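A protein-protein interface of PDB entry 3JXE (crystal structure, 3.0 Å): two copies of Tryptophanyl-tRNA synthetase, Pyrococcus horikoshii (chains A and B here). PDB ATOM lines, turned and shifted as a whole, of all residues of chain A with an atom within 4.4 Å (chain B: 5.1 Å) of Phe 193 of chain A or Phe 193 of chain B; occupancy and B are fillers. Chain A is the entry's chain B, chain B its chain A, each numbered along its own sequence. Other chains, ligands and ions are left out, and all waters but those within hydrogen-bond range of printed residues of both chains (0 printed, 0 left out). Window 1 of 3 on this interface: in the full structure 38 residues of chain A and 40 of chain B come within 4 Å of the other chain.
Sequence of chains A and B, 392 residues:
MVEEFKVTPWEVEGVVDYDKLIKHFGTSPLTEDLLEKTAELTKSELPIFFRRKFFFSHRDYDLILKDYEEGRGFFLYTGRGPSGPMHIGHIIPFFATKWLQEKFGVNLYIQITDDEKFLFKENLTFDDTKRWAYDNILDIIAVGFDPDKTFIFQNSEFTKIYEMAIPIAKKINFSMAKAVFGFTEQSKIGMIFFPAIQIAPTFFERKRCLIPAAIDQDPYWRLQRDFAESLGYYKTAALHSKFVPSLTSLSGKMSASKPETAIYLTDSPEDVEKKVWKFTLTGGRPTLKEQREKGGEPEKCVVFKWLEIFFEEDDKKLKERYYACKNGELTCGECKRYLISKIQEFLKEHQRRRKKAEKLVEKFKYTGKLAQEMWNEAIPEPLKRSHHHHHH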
ATOM      1  N   TYR A 162      -9.079   7.207  -8.691  1.00  0.00           N
ATOM      2  CA  TYR A 162      -9.334   7.422 -10.108  1.00  0.00           C
ATOM      3  C   TYR A 162      -9.139   8.897 -10.465  1.00  0.00           C
ATOM      4  O   TYR A 162      -8.449   9.216 -11.431  1.00  0.00           O
ATOM      5  CB  TYR A 162     -10.726   6.941 -10.522  1.00  0.00           C
ATOM      6  CG  TYR A 162     -11.026   7.217 -11.978  1.00  0.00           C
ATOM      7  CD1 TYR A 162     -11.986   8.160 -12.346  1.00  0.00           C
ATOM      8  CD2 TYR A 162     -10.324   6.561 -12.989  1.00  0.00           C
ATOM      9  CE1 TYR A 162     -12.254   8.426 -13.684  1.00  0.00           C
ATOM     10  CE2 TYR A 162     -10.583   6.817 -14.325  1.00  0.00           C
ATOM     11  CZ  TYR A 162     -11.547   7.749 -14.666  1.00  0.00           C
ATOM     12  OH  TYR A 162     -11.800   8.003 -15.992  1.00  0.00           O
ATOM     13  N   ALA A 165      -5.584   9.765 -10.253  1.00  0.00           N
ATOM     14  CA  ALA A 165      -4.752   9.139 -11.284  1.00  0.00           C
ATOM     15  C   ALA A 165      -4.803   9.868 -12.626  1.00  0.00           C
ATOM     16  O   ALA A 165      -3.855   9.794 -13.411  1.00  0.00           O
ATOM     17  CB  ALA A 165      -5.145   7.683 -11.468  1.00  0.00           C
ATOM     18  N   ALA A 169      -2.322   9.964 -15.879  1.00  0.00           N
ATOM     19  CA  ALA A 169      -2.877   9.134 -16.946  1.00  0.00           C
ATOM     20  C   ALA A 169      -2.892   9.887 -18.279  1.00  0.00           C
ATOM     21  O   ALA A 169      -3.094   9.288 -19.337  1.00  0.00           O
ATOM     22  CB  ALA A 169      -4.269   8.656 -16.581  1.00  0.00           C
ATOM     23  N   ILE A 189      -7.557  -3.104 -21.554  1.00  0.00           N
ATOM     24  CA  ILE A 189      -7.448  -1.650 -21.367  1.00  0.00           C
ATOM     25  C   ILE A 189      -7.279  -1.236 -19.899  1.00  0.00           C
ATOM     26  O   ILE A 189      -6.583  -0.265 -19.601  1.00  0.00           O
ATOM     27  CB  ILE A 189      -8.606  -0.861 -22.047  1.00  0.00           C
ATOM     28  CG1 ILE A 189      -9.974  -1.277 -21.493  1.00  0.00           C
ATOM     29  CG2 ILE A 189      -8.550  -1.038 -23.562  1.00  0.00           C
ATOM     30  CD1 ILE A 189     -11.116  -0.370 -21.914  1.00  0.00           C
ATOM     31  N   GLY A 190      -7.899  -1.995 -18.994  1.00  0.00           N
ATOM     32  CA  GLY A 190      -7.766  -1.777 -17.554  1.00  0.00           C
ATOM     33  C   GLY A 190      -6.370  -2.068 -17.035  1.00  0.00           C
ATOM     34  O   GLY A 190      -5.934  -1.473 -16.047  1.00  0.00           O
ATOM     35  N   MET A 191      -5.674  -2.988 -17.701  1.00  0.00           N
ATOM     36  CA  MET A 191      -4.286  -3.307 -17.372  1.00  0.00           C
ATOM     37  C   MET A 191      -3.382  -2.130 -17.712  1.00  0.00           C
ATOM     38  O   MET A 191      -2.504  -1.759 -16.933  1.00  0.00           O
ATOM     39  CB  MET A 191      -3.812  -4.547 -18.136  1.00  0.00           C
ATOM     40  CG  MET A 191      -4.421  -5.861 -17.683  1.00  0.00           C
ATOM     41  SD  MET A 191      -3.332  -7.244 -18.073  1.00  0.00           S
ATOM     42  CE  MET A 191      -4.031  -7.893 -19.571  1.00  0.00           C
ATOM     43  N   ILE A 192      -3.616  -1.550 -18.886  1.00  0.00           N
ATOM     44  CA  ILE A 192      -2.808  -0.448 -19.403  1.00  0.00           C
ATOM     45  C   ILE A 192      -2.980   0.825 -18.574  1.00  0.00           C
ATOM     46  O   ILE A 192      -2.032   1.592 -18.399  1.00  0.00           O
ATOM     47  CB  ILE A 192      -3.111  -0.209 -20.907  1.00  0.00           C
ATOM     48  CG1 ILE A 192      -2.478  -1.333 -21.736  1.00  0.00           C
ATOM     49  CG2 ILE A 192      -2.610   1.160 -21.377  1.00  0.00           C
ATOM     50  CD1 ILE A 192      -2.988  -1.434 -23.145  1.00  0.00           C
ATOM     51  N   PHE A 193      -4.186   1.027 -18.052  1.00  0.00           N
ATOM     52  CA  PHE A 193      -4.482   2.196 -17.232  1.00  0.00           C
ATOM     53  C   PHE A 193      -3.906   2.084 -15.829  1.00  0.00           C
ATOM     54  O   PHE A 193      -3.518   3.090 -15.233  1.00  0.00           O
ATOM     55  CB  PHE A 193      -5.989   2.414 -17.148  1.00  0.00           C
ATOM     56  CG  PHE A 193      -6.385   3.612 -16.327  1.00  0.00           C
ATOM     57  CD1 PHE A 193      -6.938   3.450 -15.063  1.00  0.00           C
ATOM     58  CD2 PHE A 193      -6.203   4.901 -16.817  1.00  0.00           C
ATOM     59  CE1 PHE A 193      -7.305   4.552 -14.299  1.00  0.00           C
ATOM     60  CE2 PHE A 193      -6.567   6.008 -16.062  1.00  0.00           C
ATOM     61  CZ  PHE A 193      -7.117   5.834 -14.799  1.00  0.00           C
ATOM     62  N   PHE A 194      -3.841   0.858 -15.312  1.00  0.00           N
ATOM     63  CA  PHE A 194      -3.531   0.625 -13.902  1.00  0.00           C
ATOM     64  C   PHE A 194      -2.285   1.321 -13.323  1.00  0.00           C
ATOM     65  O   PHE A 194      -2.329   1.768 -12.179  1.00  0.00           O
ATOM     66  CB  PHE A 194      -3.508  -0.870 -13.556  1.00  0.00           C
ATOM     67  CG  PHE A 194      -3.100  -1.139 -12.138  1.00  0.00           C
ATOM     68  CD1 PHE A 194      -1.812  -1.574 -11.843  1.00  0.00           C
ATOM     69  CD2 PHE A 194      -3.984  -0.902 -11.089  1.00  0.00           C
ATOM     70  CE1 PHE A 194      -1.420  -1.793 -10.531  1.00  0.00           C
ATOM     71  CE2 PHE A 194      -3.600  -1.118  -9.774  1.00  0.00           C
ATOM     72  CZ  PHE A 194      -2.313  -1.565  -9.494  1.00  0.00           C
ATOM     73  N   PRO A 195      -1.171   1.401 -14.086  1.00  0.00           N
ATOM     74  CA  PRO A 195       0.001   2.094 -13.532  1.00  0.00           C
ATOM     75  C   PRO A 195      -0.307   3.489 -12.975  1.00  0.00           C
ATOM     76  O   PRO A 195       0.323   3.912 -12.003  1.00  0.00           O
ATOM     77  CB  PRO A 195       0.943   2.192 -14.731  1.00  0.00           C
ATOM     78  CG  PRO A 195       0.599   1.018 -15.556  1.00  0.00           C
ATOM     79  CD  PRO A 195      -0.888   0.863 -15.430  1.00  0.00           C
ATOM     80  N   ALA A 196      -1.272   4.183 -13.579  1.00  0.00           N
ATOM     81  CA  ALA A 196      -1.723   5.485 -13.084  1.00  0.00           C
ATOM     82  C   ALA A 196      -2.338   5.374 -11.686  1.00  0.00           C
ATOM     83  O   ALA A 196      -2.161   6.265 -10.853  1.00  0.00           O
ATOM     84  CB  ALA A 196      -2.709   6.115 -14.056  1.00  0.00           C
ATOM     85  N   ILE A 197      -3.048   4.274 -11.441  1.00  0.00           N
ATOM     86  CA  ILE A 197      -3.678   4.003 -10.149  1.00  0.00           C
ATOM     87  C   ILE A 197      -2.648   3.722  -9.045  1.00  0.00           C
ATOM     88  O   ILE A 197      -2.792   4.219  -7.929  1.00  0.00           O
ATOM     89  CB  ILE A 197      -4.711   2.841 -10.256  1.00  0.00           C
ATOM     90  CG1 ILE A 197      -5.863   3.215 -11.202  1.00  0.00           C
ATOM     91  CG2 ILE A 197      -5.235   2.419  -8.884  1.00  0.00           C
ATOM     92  CD1 ILE A 197      -6.826   4.279 -10.673  1.00  0.00           C
ATOM     93  N   TYR B 162     -15.520   4.247 -11.957  1.00  0.00           N
ATOM     94  CA  TYR B 162     -14.281   3.488 -12.086  1.00  0.00           C
ATOM     95  C   TYR B 162     -14.502   2.031 -11.686  1.00  0.00           C
ATOM     96  O   TYR B 162     -14.090   1.118 -12.401  1.00  0.00           O
ATOM     97  CB  TYR B 162     -13.149   4.108 -11.263  1.00  0.00           C
ATOM     98  CG  TYR B 162     -11.875   3.288 -11.294  1.00  0.00           C
ATOM     99  CD1 TYR B 162     -11.143   3.145 -12.474  1.00  0.00           C
ATOM    100  CD2 TYR B 162     -11.408   2.644 -10.148  1.00  0.00           C
ATOM    101  CE1 TYR B 162      -9.981   2.392 -12.512  1.00  0.00           C
ATOM    102  CE2 TYR B 162     -10.240   1.888 -10.176  1.00  0.00           C
ATOM    103  CZ  TYR B 162      -9.535   1.766 -11.363  1.00  0.00           C
ATOM    104  OH  TYR B 162      -8.380   1.020 -11.405  1.00  0.00           O
ATOM    105  N   ALA B 165     -16.618   0.364 -14.163  1.00  0.00           N
ATOM    106  CA  ALA B 165     -15.958   0.186 -15.461  1.00  0.00           C
ATOM    107  C   ALA B 165     -14.976  -0.983 -15.498  1.00  0.00           C
ATOM    108  O   ALA B 165     -14.658  -1.494 -16.570  1.00  0.00           O
ATOM    109  CB  ALA B 165     -15.250   1.468 -15.869  1.00  0.00           C
ATOM    110  N   ALA B 169     -13.457  -3.278 -18.477  1.00  0.00           N
ATOM    111  CA  ALA B 169     -12.055  -2.927 -18.713  1.00  0.00           C
ATOM    112  C   ALA B 169     -11.158  -4.162 -18.775  1.00  0.00           C
ATOM    113  O   ALA B 169     -10.037  -4.099 -19.283  1.00  0.00           O
ATOM    114  CB  ALA B 169     -11.562  -1.962 -17.648  1.00  0.00           C
ATOM    115  N   ILE B 189      -2.536   6.652 -21.624  1.00  0.00           N
ATOM    116  CA  ILE B 189      -3.132   5.484 -20.966  1.00  0.00           C
ATOM    117  C   ILE B 189      -4.548   5.778 -20.461  1.00  0.00           C
ATOM    118  O   ILE B 189      -5.410   4.895 -20.467  1.00  0.00           O
ATOM    119  CB  ILE B 189      -2.231   4.881 -19.849  1.00  0.00           C
ATOM    120  CG1 ILE B 189      -1.920   5.912 -18.758  1.00  0.00           C
ATOM    121  CG2 ILE B 189      -0.950   4.313 -20.455  1.00  0.00           C
ATOM    122  CD1 ILE B 189      -1.245   5.332 -17.524  1.00  0.00           C
ATOM    123  N   GLY B 190      -4.780   7.026 -20.053  1.00  0.00           N
ATOM    124  CA  GLY B 190      -6.107   7.488 -19.655  1.00  0.00           C
ATOM    125  C   GLY B 190      -7.078   7.504 -20.820  1.00  0.00           C
ATOM    126  O   GLY B 190      -8.266   7.219 -20.650  1.00  0.00           O
ATOM    127  N   MET B 191      -6.566   7.837 -22.003  1.00  0.00           N
ATOM    128  CA  MET B 191      -7.355   7.832 -23.233  1.00  0.00           C
ATOM    129  C   MET B 191      -7.828   6.421 -23.570  1.00  0.00           C
ATOM    130  O   MET B 191      -8.998   6.211 -23.899  1.00  0.00           O
ATOM    131  CB  MET B 191      -6.543   8.398 -24.404  1.00  0.00           C
ATOM    132  CG  MET B 191      -6.428   9.912 -24.437  1.00  0.00           C
ATOM    133  SD  MET B 191      -6.002  10.501 -26.090  1.00  0.00           S
ATOM    134  CE  MET B 191      -4.279  10.933 -25.916  1.00  0.00           C
ATOM    135  N   ILE B 192      -6.908   5.464 -23.473  1.00  0.00           N
ATOM    136  CA  ILE B 192      -7.176   4.064 -23.806  1.00  0.00           C
ATOM    137  C   ILE B 192      -8.177   3.423 -22.844  1.00  0.00           C
ATOM    138  O   ILE B 192      -8.989   2.586 -23.246  1.00  0.00           O
ATOM    139  CB  ILE B 192      -5.859   3.249 -23.863  1.00  0.00           C
ATOM    140  CG1 ILE B 192      -5.002   3.731 -25.037  1.00  0.00           C
ATOM    141  CG2 ILE B 192      -6.132   1.745 -23.973  1.00  0.00           C
ATOM    142  CD1 ILE B 192      -3.564   3.292 -24.972  1.00  0.00           C
ATOM    143  N   PHE B 193      -8.123   3.831 -21.580  1.00  0.00           N
ATOM    144  CA  PHE B 193      -9.019   3.300 -20.558  1.00  0.00           C
ATOM    145  C   PHE B 193     -10.429   3.872 -20.655  1.00  0.00           C
ATOM    146  O   PHE B 193     -11.397   3.185 -20.330  1.00  0.00           O
ATOM    147  CB  PHE B 193      -8.449   3.565 -19.166  1.00  0.00           C
ATOM    148  CG  PHE B 193      -9.317   3.064 -18.040  1.00  0.00           C
ATOM    149  CD1 PHE B 193     -10.058   3.952 -17.268  1.00  0.00           C
ATOM    150  CD2 PHE B 193      -9.389   1.705 -17.748  1.00  0.00           C
ATOM    151  CE1 PHE B 193     -10.858   3.496 -16.226  1.00  0.00           C
ATOM    152  CE2 PHE B 193     -10.186   1.243 -16.706  1.00  0.00           C
ATOM    153  CZ  PHE B 193     -10.924   2.139 -15.946  1.00  0.00           C
ATOM    154  N   PHE B 194     -10.538   5.118 -21.114  1.00  0.00           N
ATOM    155  CA  PHE B 194     -11.806   5.850 -21.066  1.00  0.00           C
ATOM    156  C   PHE B 194     -13.051   5.130 -21.617  1.00  0.00           C
ATOM    157  O   PHE B 194     -14.118   5.242 -21.019  1.00  0.00           O
ATOM    158  CB  PHE B 194     -11.692   7.259 -21.667  1.00  0.00           C
ATOM    159  CG  PHE B 194     -13.001   7.996 -21.695  1.00  0.00           C
ATOM    160  CD1 PHE B 194     -13.525   8.555 -20.531  1.00  0.00           C
ATOM    161  CD2 PHE B 194     -13.735   8.095 -22.874  1.00  0.00           C
ATOM    162  CE1 PHE B 194     -14.748   9.214 -20.546  1.00  0.00           C
ATOM    163  CE2 PHE B 194     -14.958   8.753 -22.897  1.00  0.00           C
ATOM    164  CZ  PHE B 194     -15.465   9.313 -21.733  1.00  0.00           C
ATOM    165  N   PRO B 195     -12.939   4.423 -22.763  1.00  0.00           N
ATOM    166  CA  PRO B 195     -14.139   3.743 -23.268  1.00  0.00           C
ATOM    167  C   PRO B 195     -14.863   2.889 -22.221  1.00  0.00           C
ATOM    168  O   PRO B 195     -16.086   2.753 -22.282  1.00  0.00           O
ATOM    169  CB  PRO B 195     -13.591   2.867 -24.394  1.00  0.00           C
ATOM    170  CG  PRO B 195     -12.416   3.615 -24.887  1.00  0.00           C
ATOM    171  CD  PRO B 195     -11.790   4.223 -23.667  1.00  0.00           C
ATOM    172  N   ALA B 196     -14.117   2.333 -21.267  1.00  0.00           N
ATOM    173  CA  ALA B 196     -14.711   1.582 -20.162  1.00  0.00           C
ATOM    174  C   ALA B 196     -15.585   2.483 -19.284  1.00  0.00           C
ATOM    175  O   ALA B 196     -16.636   2.056 -18.803  1.00  0.00           O
ATOM    176  CB  ALA B 196     -13.631   0.909 -19.331  1.00  0.00           C
ATOM    177  N   ILE B 197     -15.145   3.725 -19.095  1.00  0.00           N
ATOM    178  CA  ILE B 197     -15.871   4.722 -18.307  1.00  0.00           C
ATOM    179  C   ILE B 197     -17.189   5.150 -18.971  1.00  0.00           C
ATOM    180  O   ILE B 197     -18.205   5.286 -18.290  1.00  0.00           O
ATOM    181  CB  ILE B 197     -14.971   5.958 -17.995  1.00  0.00           C
ATOM    182  CG1 ILE B 197     -13.765   5.557 -17.129  1.00  0.00           C
ATOM    183  CG2 ILE B 197     -15.767   7.105 -17.363  1.00  0.00           C
ATOM    184  CD1 ILE B 197     -14.096   5.162 -15.687  1.00  0.00           C
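The backbone NH (N) of Gly 190 of chain B sits at hydrogen-bond distance from the backbone carbonyl oxygen (O) of Ala 169 of chain A (2.9 Å).
The backbone carbonyl oxygen (O) of Ala 169 of chain B sits at hydrogen-bond distance from the backbone NH (N) of Gly 190 of chain A.
Among the printed residues, pairs that only touch across the chains: Tyr 162 of chain A with Tyr 162 of chain B (3.6 Å), Tyr 162 of chain A with Phe 193 of chain B (3.8 Å), Tyr 162 of chain A with Ile 197 of chain B (3.3 Å), Ala 169 of chain A with Ile 189 of chain B (3.5 Å), Ile 189 of chain A with Ala 169 of chain B (3.5 Å), Ile 189 of chain A with Ile 192 of chain B (3.7 Å), Ile 189 of chain A with Phe 193 of chain B (3.9 Å), Ile 189 of chain A with Ala 196 of chain B (3.8 Å), Gly 190 of chain A with Phe 193 of chain B (3.8 Å), Ile 192 of chain A with Ile 189 of chain B (3.6 Å), Phe 193 of chain A with Tyr 162 of chain B (3.9 Å), Phe 193 of chain A with Ile 189 of chain B (3.7 Å), Phe 193 of chain A with Gly 190 of chain B (3.8 Å), Phe 193 of chain A with Phe 193 of chain B (3.4 Å), Ala 196 of chain A with Ile 189 of chain B (3.8 Å) and Ile 197 of chain A with Tyr 162 of chain B (3.3 Å).
Of chain B, only Tyr 162, Ile 189, Gly 190 and Phe 193 come within 4 Å of Phe 193 of chain A.
Of chain A, only Tyr 162 (3.8 Å), Ile 189 (3.9 Å), Gly 190 (3.8 Å) and Phe 193 (3.4 Å) come within 4 Å of Phe 193 of chain B.
Of the printed residues of chain A, Ala 169 of chain B touches Ile 189 (3.5 Å) and Gly 190 (3.0 Å).
Printed residues of chain B within 4 Å of Tyr 162 of chain A: Tyr 162 (3.6 Å), Phe 193 (3.8 Å) and Ile 197 (3.3 Å).
Met 191 of chain A touches none of the printed residues of chain B.
Met 191 of chain B touches none of the printed residues of chain A.
The nearest printed residue of chain A that does not touch Phe 193 of chain B is Met 191 of chain A (6.0 Å).
Along chain B the printed residues that touch a printed residue of chain A span positions 162 to 197.
Of the 12 printed residues of chain A, 8 touch a printed residue of chain B.
Among the printed residues, no Asp or Glu carboxylate lies within 4 Å of a Lys or Arg side-chain nitrogen of the other chain.
Tyr 162 of chain B touches its own counterpart, Tyr 162 of chain A.
Tyr 162 of chain A touches Ile 197 of chain B, and with the chains exchanged Ile 197 of chain A touches Tyr 162 of chain B.
Ile 189 of chain A touches Ile 192 of chain B, and with the chains exchanged Ile 192 of chain A touches Ile 189 of chain B.
Gly 190 of chain A touches Phe 193 of chain B, and with the chains exchanged Phe 193 of chain A touches Gly 190 of chain B.
Of the 18 pairs that touch across the chains among the printed residues, 18 have their exchanged pair printed and touching as well.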
